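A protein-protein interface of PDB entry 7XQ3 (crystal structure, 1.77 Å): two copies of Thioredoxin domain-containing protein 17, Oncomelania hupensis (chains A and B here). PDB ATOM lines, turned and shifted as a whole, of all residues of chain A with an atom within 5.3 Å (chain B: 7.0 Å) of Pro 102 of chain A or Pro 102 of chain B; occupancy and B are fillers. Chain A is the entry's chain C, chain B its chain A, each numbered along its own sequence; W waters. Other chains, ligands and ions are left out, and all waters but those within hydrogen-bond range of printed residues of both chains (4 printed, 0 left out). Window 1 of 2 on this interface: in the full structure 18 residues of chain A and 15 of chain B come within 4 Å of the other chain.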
ATOM      1  N   GLY A 100     -14.200 -20.831  -8.077  1.00  0.00           N
ATOM      2  CA  GLY A 100     -13.369 -21.483  -7.056  1.00  0.00           C
ATOM      3  C   GLY A 100     -11.904 -21.428  -7.430  1.00  0.00           C
ATOM      4  O   GLY A 100     -11.088 -22.255  -6.899  1.00  0.00           O
ATOM      5  N   THR A 101     -11.547 -20.520  -8.338  1.00  0.00           N
ATOM      6  CA  THR A 101     -10.146 -20.424  -8.831  1.00  0.00           C
ATOM      7  C   THR A 101      -9.774 -18.959  -8.897  1.00  0.00           C
ATOM      8  O   THR A 101     -10.643 -18.087  -8.848  1.00  0.00           O
ATOM      9  CB  THR A 101      -9.929 -21.080 -10.200  1.00  0.00           C
ATOM     10  OG1 THR A 101     -10.365 -20.149 -11.206  1.00  0.00           O
ATOM     11  CG2 THR A 101     -10.580 -22.438 -10.327  1.00  0.00           C
ATOM     12  N   PRO A 102      -8.483 -18.618  -9.086  1.00  0.00           N
ATOM     13  CA  PRO A 102      -8.128 -17.225  -9.374  1.00  0.00           C
ATOM     14  C   PRO A 102      -8.425 -16.741 -10.812  1.00  0.00           C
ATOM     15  O   PRO A 102      -8.105 -15.615 -11.169  1.00  0.00           O
ATOM     16  CB  PRO A 102      -6.610 -17.225  -9.055  1.00  0.00           C
ATOM     17  CG  PRO A 102      -6.301 -18.575  -8.441  1.00  0.00           C
ATOM     18  CD  PRO A 102      -7.323 -19.517  -9.035  1.00  0.00           C
ATOM     19  N   GLN A 103      -9.008 -17.587 -11.677  1.00  0.00           N
ATOM     20  CA  GLN A 103      -9.156 -17.243 -13.117  1.00  0.00           C
ATOM     21  C   GLN A 103     -10.382 -16.345 -13.304  1.00  0.00           C
ATOM     22  O   GLN A 103     -11.478 -16.858 -13.163  1.00  0.00           O
ATOM     23  CB  GLN A 103      -9.220 -18.527 -13.925  1.00  0.00           C
ATOM     24  CG  GLN A 103      -7.927 -19.317 -13.829  1.00  0.00           C
ATOM     25  CD  GLN A 103      -7.964 -20.627 -14.577  1.00  0.00           C
ATOM     26  OE1 GLN A 103      -8.130 -21.711 -13.992  1.00  0.00           O
ATOM     27  NE2 GLN A 103      -7.816 -20.529 -15.891  1.00  0.00           N
ATOM     28  N   ARG A 104     -10.200 -15.036 -13.509  1.00  0.00           N
ATOM     29  CA  ARG A 104     -11.327 -14.062 -13.584  1.00  0.00           C
ATOM     30  C   ARG A 104     -11.009 -12.927 -14.579  1.00  0.00           C
ATOM     31  O   ARG A 104      -9.919 -12.326 -14.514  1.00  0.00           O
ATOM     32  CB  ARG A 104     -11.591 -13.418 -12.214  1.00  0.00           C
ATOM     33  CG  ARG A 104     -12.899 -12.631 -12.113  1.00  0.00           C
ATOM     34  CD  ARG A 104     -13.126 -12.006 -10.740  1.00  0.00           C
ATOM     35  NE  ARG A 104     -13.182 -13.027  -9.691  1.00  0.00           N
ATOM     36  CZ  ARG A 104     -14.256 -13.347  -8.985  1.00  0.00           C
ATOM     37  NH1 ARG A 104     -15.414 -12.724  -9.153  1.00  0.00           N
ATOM     38  NH2 ARG A 104     -14.171 -14.345  -8.131  1.00  0.00           N
ATOM     39  N   LEU A 105     -11.964 -12.561 -15.397  1.00  0.00           N
ATOM     40  CA  LEU A 105     -11.874 -11.347 -16.254  1.00  0.00           C
ATOM     41  C   LEU A 105     -13.107 -10.499 -16.026  1.00  0.00           C
ATOM     42  O   LEU A 105     -14.199 -11.074 -15.868  1.00  0.00           O
ATOM     43  CB  LEU A 105     -11.815 -11.709 -17.744  1.00  0.00           C
ATOM     44  CG  LEU A 105     -10.630 -12.539 -18.196  1.00  0.00           C
ATOM     45  CD1 LEU A 105     -10.793 -12.943 -19.644  1.00  0.00           C
ATOM     46  CD2 LEU A 105      -9.320 -11.759 -17.994  1.00  0.00           C
ATOM     47  N   LEU A 115      -6.811 -12.349 -23.881  1.00  0.00           N
ATOM     48  CA  LEU A 115      -7.053 -12.724 -22.462  1.00  0.00           C
ATOM     49  C   LEU A 115      -8.190 -13.764 -22.411  1.00  0.00           C
ATOM     50  O   LEU A 115      -8.110 -14.697 -21.611  1.00  0.00           O
ATOM     51  CB  LEU A 115      -7.443 -11.522 -21.603  1.00  0.00           C
ATOM     52  CG  LEU A 115      -6.309 -10.550 -21.249  1.00  0.00           C
ATOM     53  CD1 LEU A 115      -6.860  -9.406 -20.442  1.00  0.00           C
ATOM     54  CD2 LEU A 115      -5.189 -11.302 -20.526  1.00  0.00           C
ATOM     55  N   MET A 118      -6.711 -17.056 -23.514  1.00  0.00           N
ATOM     56  CA  MET A 118      -5.862 -17.548 -22.378  1.00  0.00           C
ATOM     57  C   MET A 118      -6.751 -18.159 -21.292  1.00  0.00           C
ATOM     58  O   MET A 118      -6.409 -19.235 -20.781  1.00  0.00           O
ATOM     59  CB  MET A 118      -5.027 -16.409 -21.784  1.00  0.00           C
ATOM     60  CG  MET A 118      -3.933 -15.899 -22.672  1.00  0.00           C
ATOM     61  SD  MET A 118      -2.949 -14.540 -21.869  1.00  0.00           S
ATOM     62  CE  MET A 118      -3.085 -15.124 -20.189  1.00  0.00           C
ATOM     63  N   PHE A 119      -7.880 -17.524 -20.994  1.00  0.00           N
ATOM     64  CA  PHE A 119      -8.837 -17.923 -19.935  1.00  0.00           C
ATOM     65  C   PHE A 119      -9.361 -19.319 -20.277  1.00  0.00           C
ATOM     66  O   PHE A 119      -9.425 -20.197 -19.411  1.00  0.00           O
ATOM     67  CB  PHE A 119      -9.937 -16.860 -19.872  1.00  0.00           C
ATOM     68  CG  PHE A 119     -11.140 -17.228 -19.041  1.00  0.00           C
ATOM     69  CD1 PHE A 119     -11.091 -17.075 -17.674  1.00  0.00           C
ATOM     70  CD2 PHE A 119     -12.243 -17.859 -19.602  1.00  0.00           C
ATOM     71  CE1 PHE A 119     -12.174 -17.416 -16.876  1.00  0.00           C
ATOM     72  CE2 PHE A 119     -13.329 -18.206 -18.808  1.00  0.00           C
ATOM     73  CZ  PHE A 119     -13.282 -17.993 -17.440  1.00  0.00           C
ATOM     74  N   LEU B  96      -3.766  -9.475  -5.836  1.00  0.00           N
ATOM     75  CA  LEU B  96      -2.728 -10.443  -6.236  1.00  0.00           C
ATOM     76  C   LEU B  96      -2.950 -10.765  -7.722  1.00  0.00           C
ATOM     77  O   LEU B  96      -4.036 -11.196  -8.058  1.00  0.00           O
ATOM     78  CB  LEU B  96      -2.943 -11.670  -5.356  1.00  0.00           C
ATOM     79  CG  LEU B  96      -1.872 -12.041  -4.349  1.00  0.00           C
ATOM     80  CD1 LEU B  96      -2.202 -13.455  -3.872  1.00  0.00           C
ATOM     81  CD2 LEU B  96      -0.448 -12.013  -4.933  1.00  0.00           C
ATOM     82  N   LYS B  98      -1.062 -12.062 -11.706  1.00  0.00           N
ATOM     83  CA  LYS B  98       0.003 -12.315 -12.702  1.00  0.00           C
ATOM     84  C   LYS B  98      -0.270 -11.373 -13.850  1.00  0.00           C
ATOM     85  O   LYS B  98      -1.278 -11.509 -14.543  1.00  0.00           O
ATOM     86  CB  LYS B  98      -0.009 -13.755 -13.207  1.00  0.00           C
ATOM     87  CG  LYS B  98       0.222 -14.804 -12.144  1.00  0.00           C
ATOM     88  CD  LYS B  98       0.686 -16.148 -12.700  1.00  0.00           C
ATOM     89  CE  LYS B  98       0.193 -16.481 -14.109  1.00  0.00           C
ATOM     90  NZ  LYS B  98       1.116 -16.040 -15.190  1.00  0.00           N
ATOM     91  N   PRO B  99       0.553 -10.326 -14.031  1.00  0.00           N
ATOM     92  CA  PRO B  99       0.246  -9.307 -15.018  1.00  0.00           C
ATOM     93  C   PRO B  99       0.123  -9.914 -16.408  1.00  0.00           C
ATOM     94  O   PRO B  99       0.906 -10.781 -16.754  1.00  0.00           O
ATOM     95  CB  PRO B  99       1.424  -8.331 -14.997  1.00  0.00           C
ATOM     96  CG  PRO B  99       2.123  -8.628 -13.679  1.00  0.00           C
ATOM     97  CD  PRO B  99       1.790 -10.049 -13.293  1.00  0.00           C
ATOM     98  N   GLY B 100      -0.937  -9.481 -17.081  1.00  0.00           N
ATOM     99  CA  GLY B 100      -1.255  -9.819 -18.471  1.00  0.00           C
ATOM    100  C   GLY B 100      -1.926 -11.175 -18.584  1.00  0.00           C
ATOM    101  O   GLY B 100      -1.890 -11.744 -19.693  1.00  0.00           O
ATOM    102  N   THR B 101      -2.464 -11.695 -17.484  1.00  0.00           N
ATOM    103  CA  THR B 101      -3.190 -12.981 -17.469  1.00  0.00           C
ATOM    104  C   THR B 101      -4.534 -12.818 -16.787  1.00  0.00           C
ATOM    105  O   THR B 101      -4.820 -11.826 -16.139  1.00  0.00           O
ATOM    106  CB  THR B 101      -2.396 -14.097 -16.775  1.00  0.00           C
ATOM    107  OG1 THR B 101      -2.566 -13.900 -15.369  1.00  0.00           O
ATOM    108  CG2 THR B 101      -0.927 -14.163 -17.152  1.00  0.00           C
ATOM    109  N   PRO B 102      -5.421 -13.835 -16.854  1.00  0.00           N
ATOM    110  CA  PRO B 102      -6.652 -13.831 -16.054  1.00  0.00           C
ATOM    111  C   PRO B 102      -6.458 -14.162 -14.560  1.00  0.00           C
ATOM    112  O   PRO B 102      -7.461 -14.242 -13.840  1.00  0.00           O
ATOM    113  CB  PRO B 102      -7.514 -14.905 -16.790  1.00  0.00           C
ATOM    114  CG  PRO B 102      -6.802 -15.094 -18.080  1.00  0.00           C
ATOM    115  CD  PRO B 102      -5.333 -14.994 -17.718  1.00  0.00           C
ATOM    116  N   GLN B 103      -5.214 -14.378 -14.092  1.00  0.00           N
ATOM    117  CA  GLN B 103      -4.952 -14.874 -12.711  1.00  0.00           C
ATOM    118  C   GLN B 103      -4.964 -13.684 -11.754  1.00  0.00           C
ATOM    119  O   GLN B 103      -4.015 -12.875 -11.797  1.00  0.00           O
ATOM    120  CB  GLN B 103      -3.626 -15.639 -12.628  1.00  0.00           C
ATOM    121  CG  GLN B 103      -3.463 -16.464 -11.361  1.00  0.00           C
ATOM    122  CD  GLN B 103      -4.034 -17.855 -11.477  1.00  0.00           C
ATOM    123  OE1 GLN B 103      -5.219 -18.066 -11.306  1.00  0.00           O
ATOM    124  NE2 GLN B 103      -3.209 -18.827 -11.837  1.00  0.00           N
ATOM    125  N   ARG B 104      -6.052 -13.523 -10.991  1.00  0.00           N
ATOM    126  CA  ARG B 104      -6.264 -12.330 -10.135  1.00  0.00           C
ATOM    127  C   ARG B 104      -7.028 -12.764  -8.884  1.00  0.00           C
ATOM    128  O   ARG B 104      -8.064 -13.461  -9.033  1.00  0.00           O
ATOM    129  CB  ARG B 104      -7.069 -11.249 -10.887  1.00  0.00           C
ATOM    130  CG  ARG B 104      -7.066  -9.875 -10.229  1.00  0.00           C
ATOM    131  CD  ARG B 104      -7.895  -8.817 -10.927  1.00  0.00           C
ATOM    132  NE  ARG B 104      -7.352  -8.513 -12.251  1.00  0.00           N
ATOM    133  CZ  ARG B 104      -6.723  -7.393 -12.585  1.00  0.00           C
ATOM    134  NH1 ARG B 104      -6.639  -6.373 -11.754  1.00  0.00           N
ATOM    135  NH2 ARG B 104      -6.217  -7.279 -13.786  1.00  0.00           N
ATOM    136  N   LEU B 105      -6.619 -12.257  -7.733  1.00  0.00           N
ATOM    137  CA  LEU B 105      -7.389 -12.321  -6.477  1.00  0.00           C
ATOM    138  C   LEU B 105      -7.498 -10.917  -5.910  1.00  0.00           C
ATOM    139  O   LEU B 105      -6.507 -10.136  -5.963  1.00  0.00           O
ATOM    140  CB  LEU B 105      -6.687 -13.253  -5.483  1.00  0.00           C
ATOM    141  CG  LEU B 105      -6.616 -14.707  -5.899  1.00  0.00           C
ATOM    142  CD1 LEU B 105      -5.801 -15.554  -4.891  1.00  0.00           C
ATOM    143  CD2 LEU B 105      -8.017 -15.267  -6.061  1.00  0.00           C
ATOM    144  N   GLN B 109     -10.125 -12.531  -0.812  1.00  0.00           N
ATOM    145  CA  GLN B 109      -9.593 -13.720  -1.546  1.00  0.00           C
ATOM    146  C   GLN B 109      -8.063 -13.769  -1.442  1.00  0.00           C
ATOM    147  O   GLN B 109      -7.491 -14.871  -1.512  1.00  0.00           O
ATOM    148  CB  GLN B 109     -10.095 -13.771  -3.003  1.00  0.00           C
ATOM    149  CG  GLN B 109     -11.615 -13.912  -3.044  1.00  0.00           C
ATOM    150  CD  GLN B 109     -12.245 -14.769  -4.116  1.00  0.00           C
ATOM    151  OE1 GLN B 109     -11.934 -14.651  -5.302  1.00  0.00           O
ATOM    152  NE2 GLN B 109     -13.278 -15.511  -3.729  1.00  0.00           N
ATOM    153  N   ASN B 114      -6.212 -21.473   0.347  1.00  0.00           N
ATOM    154  CA  ASN B 114      -6.304 -22.400  -0.803  1.00  0.00           C
ATOM    155  C   ASN B 114      -6.276 -21.643  -2.136  1.00  0.00           C
ATOM    156  O   ASN B 114      -5.518 -22.056  -3.016  1.00  0.00           O
ATOM    157  CB  ASN B 114      -7.477 -23.354  -0.638  1.00  0.00           C
ATOM    158  CG  ASN B 114      -7.380 -24.416  -1.710  1.00  0.00           C
ATOM    159  OD1 ASN B 114      -6.459 -25.245  -1.735  1.00  0.00           O
ATOM    160  ND2 ASN B 114      -8.257 -24.316  -2.655  1.00  0.00           N
ATOM    161  N   LEU B 115      -6.969 -20.521  -2.264  1.00  0.00           N
ATOM    162  CA  LEU B 115      -6.914 -19.724  -3.509  1.00  0.00           C
ATOM    163  C   LEU B 115      -5.516 -19.150  -3.678  1.00  0.00           C
ATOM    164  O   LEU B 115      -5.049 -19.116  -4.800  1.00  0.00           O
ATOM    165  CB  LEU B 115      -7.927 -18.586  -3.496  1.00  0.00           C
ATOM    166  CG  LEU B 115      -9.415 -18.962  -3.570  1.00  0.00           C
ATOM    167  CD1 LEU B 115     -10.233 -17.707  -3.477  1.00  0.00           C
ATOM    168  CD2 LEU B 115      -9.740 -19.699  -4.857  1.00  0.00           C
ATOM    169  N   VAL B 116      -4.899 -18.662  -2.615  1.00  0.00           N
ATOM    170  CA  VAL B 116      -3.501 -18.162  -2.744  1.00  0.00           C
ATOM    171  C   VAL B 116      -2.558 -19.304  -3.122  1.00  0.00           C
ATOM    172  O   VAL B 116      -1.679 -19.096  -4.010  1.00  0.00           O
ATOM    173  CB  VAL B 116      -3.038 -17.451  -1.484  1.00  0.00           C
ATOM    174  CG1 VAL B 116      -1.579 -17.073  -1.625  1.00  0.00           C
ATOM    175  CG2 VAL B 116      -3.921 -16.239  -1.194  1.00  0.00           C
ATOM    176  N   GLN B 117      -2.717 -20.483  -2.529  1.00  0.00           N
ATOM    177  CA  GLN B 117      -1.844 -21.603  -2.948  1.00  0.00           C
ATOM    178  C   GLN B 117      -2.053 -21.878  -4.442  1.00  0.00           C
ATOM    179  O   GLN B 117      -1.057 -22.031  -5.199  1.00  0.00           O
ATOM    180  CB  GLN B 117      -2.094 -22.808  -2.056  1.00  0.00           C
ATOM    181  CG  GLN B 117      -1.277 -24.022  -2.446  1.00  0.00           C
ATOM    182  CD  GLN B 117      -1.781 -25.272  -1.763  1.00  0.00           C
ATOM    183  OE1 GLN B 117      -2.237 -25.263  -0.615  1.00  0.00           O
ATOM    184  NE2 GLN B 117      -1.778 -26.359  -2.518  1.00  0.00           N
ATOM    185  N   MET B 118      -3.314 -21.965  -4.858  1.00  0.00           N
ATOM    186  CA  MET B 118      -3.683 -22.244  -6.267  1.00  0.00           C
ATOM    187  C   MET B 118      -3.077 -21.181  -7.190  1.00  0.00           C
ATOM    188  O   MET B 118      -2.588 -21.525  -8.286  1.00  0.00           O
ATOM    189  CB  MET B 118      -5.201 -22.235  -6.405  1.00  0.00           C
ATOM    190  CG  MET B 118      -5.706 -22.813  -7.698  1.00  0.00           C
ATOM    191  SD  MET B 118      -7.536 -22.853  -7.668  1.00  0.00           S
ATOM    192  CE  MET B 118      -7.863 -23.258  -5.957  1.00  0.00           C
ATOM    193  N   PHE B 119      -3.075 -19.939  -6.761  1.00  0.00           N
ATOM    194  CA  PHE B 119      -2.544 -18.820  -7.582  1.00  0.00           C
ATOM    195  C   PHE B 119      -1.058 -19.033  -7.851  1.00  0.00           C
ATOM    196  O   PHE B 119      -0.568 -18.805  -8.977  1.00  0.00           O
ATOM    197  CB  PHE B 119      -2.822 -17.530  -6.833  1.00  0.00           C
ATOM    198  CG  PHE B 119      -2.134 -16.308  -7.369  1.00  0.00           C
ATOM    199  CD1 PHE B 119      -2.713 -15.593  -8.371  1.00  0.00           C
ATOM    200  CD2 PHE B 119      -0.921 -15.879  -6.842  1.00  0.00           C
ATOM    201  CE1 PHE B 119      -2.117 -14.446  -8.868  1.00  0.00           C
ATOM    202  CE2 PHE B 119      -0.337 -14.722  -7.329  1.00  0.00           C
ATOM    203  CZ  PHE B 119      -0.905 -14.047  -8.375  1.00  0.00           C
ATOM    204  N   PHE B 120      -0.294 -19.390  -6.823  1.00  0.00           N
ATOM    205  CA  PHE B 120       1.173 -19.585  -7.001  1.00  0.00           C
ATOM    206  C   PHE B 120       1.449 -20.900  -7.748  1.00  0.00           C
ATOM    207  O   PHE B 120       2.470 -21.008  -8.485  1.00  0.00           O
ATOM    208  CB  PHE B 120       1.882 -19.492  -5.652  1.00  0.00           C
ATOM    209  CG  PHE B 120       1.973 -18.094  -5.091  1.00  0.00           C
ATOM    210  CD1 PHE B 120       2.661 -17.110  -5.794  1.00  0.00           C
ATOM    211  CD2 PHE B 120       1.435 -17.773  -3.843  1.00  0.00           C
ATOM    212  CE1 PHE B 120       2.782 -15.829  -5.274  1.00  0.00           C
ATOM    213  CE2 PHE B 120       1.554 -16.492  -3.333  1.00  0.00           C
ATOM    214  CZ  PHE B 120       2.195 -15.523  -4.049  1.00  0.00           C
HETATM  215  O   HOH W   1     -10.522 -14.267  -8.804  1.00  0.00           O
HETATM  216  O   HOH W   2      -8.353 -10.308 -14.299  1.00  0.00           O
HETATM  217  O   HOH W   3     -12.095 -16.729  -7.002  1.00  0.00           O
HETATM  218  O   HOH W   4     -10.348 -24.766  -7.796  1.00  0.00           O
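N of Leu 105 of chain B sits at hydrogen-bond distance from O of Leu 96 of chain B.
The backbone NH (N) of Lys 98 of chain B sits at hydrogen-bond distance from the backbone carbonyl oxygen (O) of Gln 103 of chain B (3.1 Å).
The side-chain hydroxyl (OG1) of Thr 101 of chain A lies within hydrogen-bond range of the backbone NH (N) of Gln 103 of chain A (2.9 Å).
The backbone carbonyl oxygen of Lys 98 of chain B is in hydrogen-bond range of the side-chain hydroxyl of Thr 101 of chain B (2.8 Å).
OG1 of Thr 101 of chain B sits at hydrogen-bond distance from N of Gln 103 of chain B (3.0 Å).
Of chain B, only Pro 102, Gln 103, Arg 104, Leu 105, Leu 115, Met 118 and Phe 119 come within 4 Å of Pro 102 of chain A.
Of chain A, only Pro 102 (3.1 Å), Gln 103 (3.5 Å), Arg 104 (2.9 Å), Leu 105 (3.8 Å), Leu 115 (3.8 Å), Met 118 (3.3 Å) and Phe 119 (3.9 Å) come within 4 Å of Pro 102 of chain B.
Printed residues of chain B within 4 Å of Leu 115 of chain A: Gly 100 and Pro 102.
Printed residues of chain A within 4 Å of Leu 105 of chain B: Pro 102.
Of the printed residues of chain A, Leu 115 of chain B touches Gly 100 (3.5 Å) and Pro 102 (3.9 Å).
Of the printed residues of chain A, Met 118 of chain B touches Gly 100, Thr 101 and Pro 102.
Printed residues of chain A within 4 Å of Arg 104 of chain B: Pro 102 (2.9 Å).
The nearest residue of chain B that does not touch Pro 102 of chain A is Val 116 of chain B (6.0 Å).
The nearest printed residue of chain A that does not touch Pro 102 of chain B is Thr 101 of chain A (7.1 Å).
The nearest printed residue of chain A that does not touch Leu 105 of chain B is Thr 101 of chain A (4.8 Å).
Water W2 lies within hydrogen-bond range of O of Arg 104 of chain A (2.6 Å) and NE of Arg 104 of chain B (2.9 Å).
Water W1 lies within hydrogen-bond range of the backbone carbonyl oxygen (O) of Arg 104 of chain B (2.6 Å) and the guanidinium group (NE) of Arg 104 of chain A (3.1 Å).
Water W3 lies within hydrogen-bond range of OE1 of Gln 109 of chain B (2.7 Å), O of Thr 101 of chain A (2.7 Å) and NH2 of Arg 104 of chain A (3.4 Å).
Water W4 lies within hydrogen-bond range of O of Gly 100 of chain A (2.8 Å) and SD of Met 118 of chain B (3.4 Å).
Of the 9 printed residues of chain A, 9 touch a printed residue of chain B.
Printed residues of chain A that touch a printed residue of chain B: Gly 100, Thr 101, Pro 102, Gln 103, Arg 104, Leu 105, Leu 115, Met 118 and Phe 119.
Along chain A the printed residues that touch a printed residue of chain B span positions 100 to 119.
Hydrophobic or aromatic side chains of chain B within 4 Å of the printed part of chain A: Pro 102, Leu 105, Leu 115, Met 118 and Phe 119.
Among the printed residues, 21 pairs touch across the chains.
Among the printed residues, no Asp or Glu carboxylate lies within 4 Å of a Lys or Arg side-chain nitrogen of the other chain.
The side-chain sulfur (SD) of Met 118 of chain B sits close to the backbone carbonyl oxygen (O) of Gly 100 of chain A (3.7 Å).
O of Pro 102 of chain B is in hydrogen-bond range of N of Arg 104 of chain A, 2.9 Å away.
The side-chain sulfur (SD) of Met 118 of chain A sits close to the backbone carbonyl oxygen (O) of Gly 100 of chain B.
The backbone carbonyl oxygen (O) of Pro 102 of chain B lies close to the backbone carbonyl oxygen (O) of Pro 102 of chain A (3.1 Å).
The backbone NH (N) of Arg 104 of chain B is in hydrogen-bond range of the backbone carbonyl oxygen (O) of Pro 102 of chain A.
CD2 of Leu 115 of chain B touches O of Gly 100 of chain A (3.5 Å).
CB of Pro 102 of chain A touches CD2 of Leu 105 of chain B, 3.8 Å away.
CG of Pro 102 of chain A touches O of Leu 115 of chain B, 3.9 Å away.
Met 118 of chain B touches Pro 102 of chain A (SD to CD, 3.6 Å).
Gln 103 of chain A touches Gln 103 of chain B.
NH2 of Arg 104 of chain A touches OE1 of Gln 109 of chain B, 3.6 Å away.
Leu 115 of chain A touches Pro 102 of chain B (O to CG, 3.8 Å).
Met 118 of chain A touches Thr 101 of chain B.
Met 118 of chain A touches Pro 102 of chain B (CE to CD, 3.3 Å).
CG of Pro 102 of chain B touches N of Phe 119 of chain A (3.9 Å).
Gly 100 of chain A touches Met 118 of chain B, and with the chains exchanged Met 118 of chain A touches Gly 100 of chain B.
Thr 101 of chain A touches Met 118 of chain B, and with the chains exchanged Met 118 of chain A touches Thr 101 of chain B.
Pro 102 of chain B touches its own counterpart, Pro 102 of chain A.
Pro 102 of chain A touches Leu 115 of chain B, and with the chains exchanged Leu 115 of chain A touches Pro 102 of chain B.
Positions printed for both chains: 100, 101, 102, 103, 104, 105, 115, 118 and 119.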
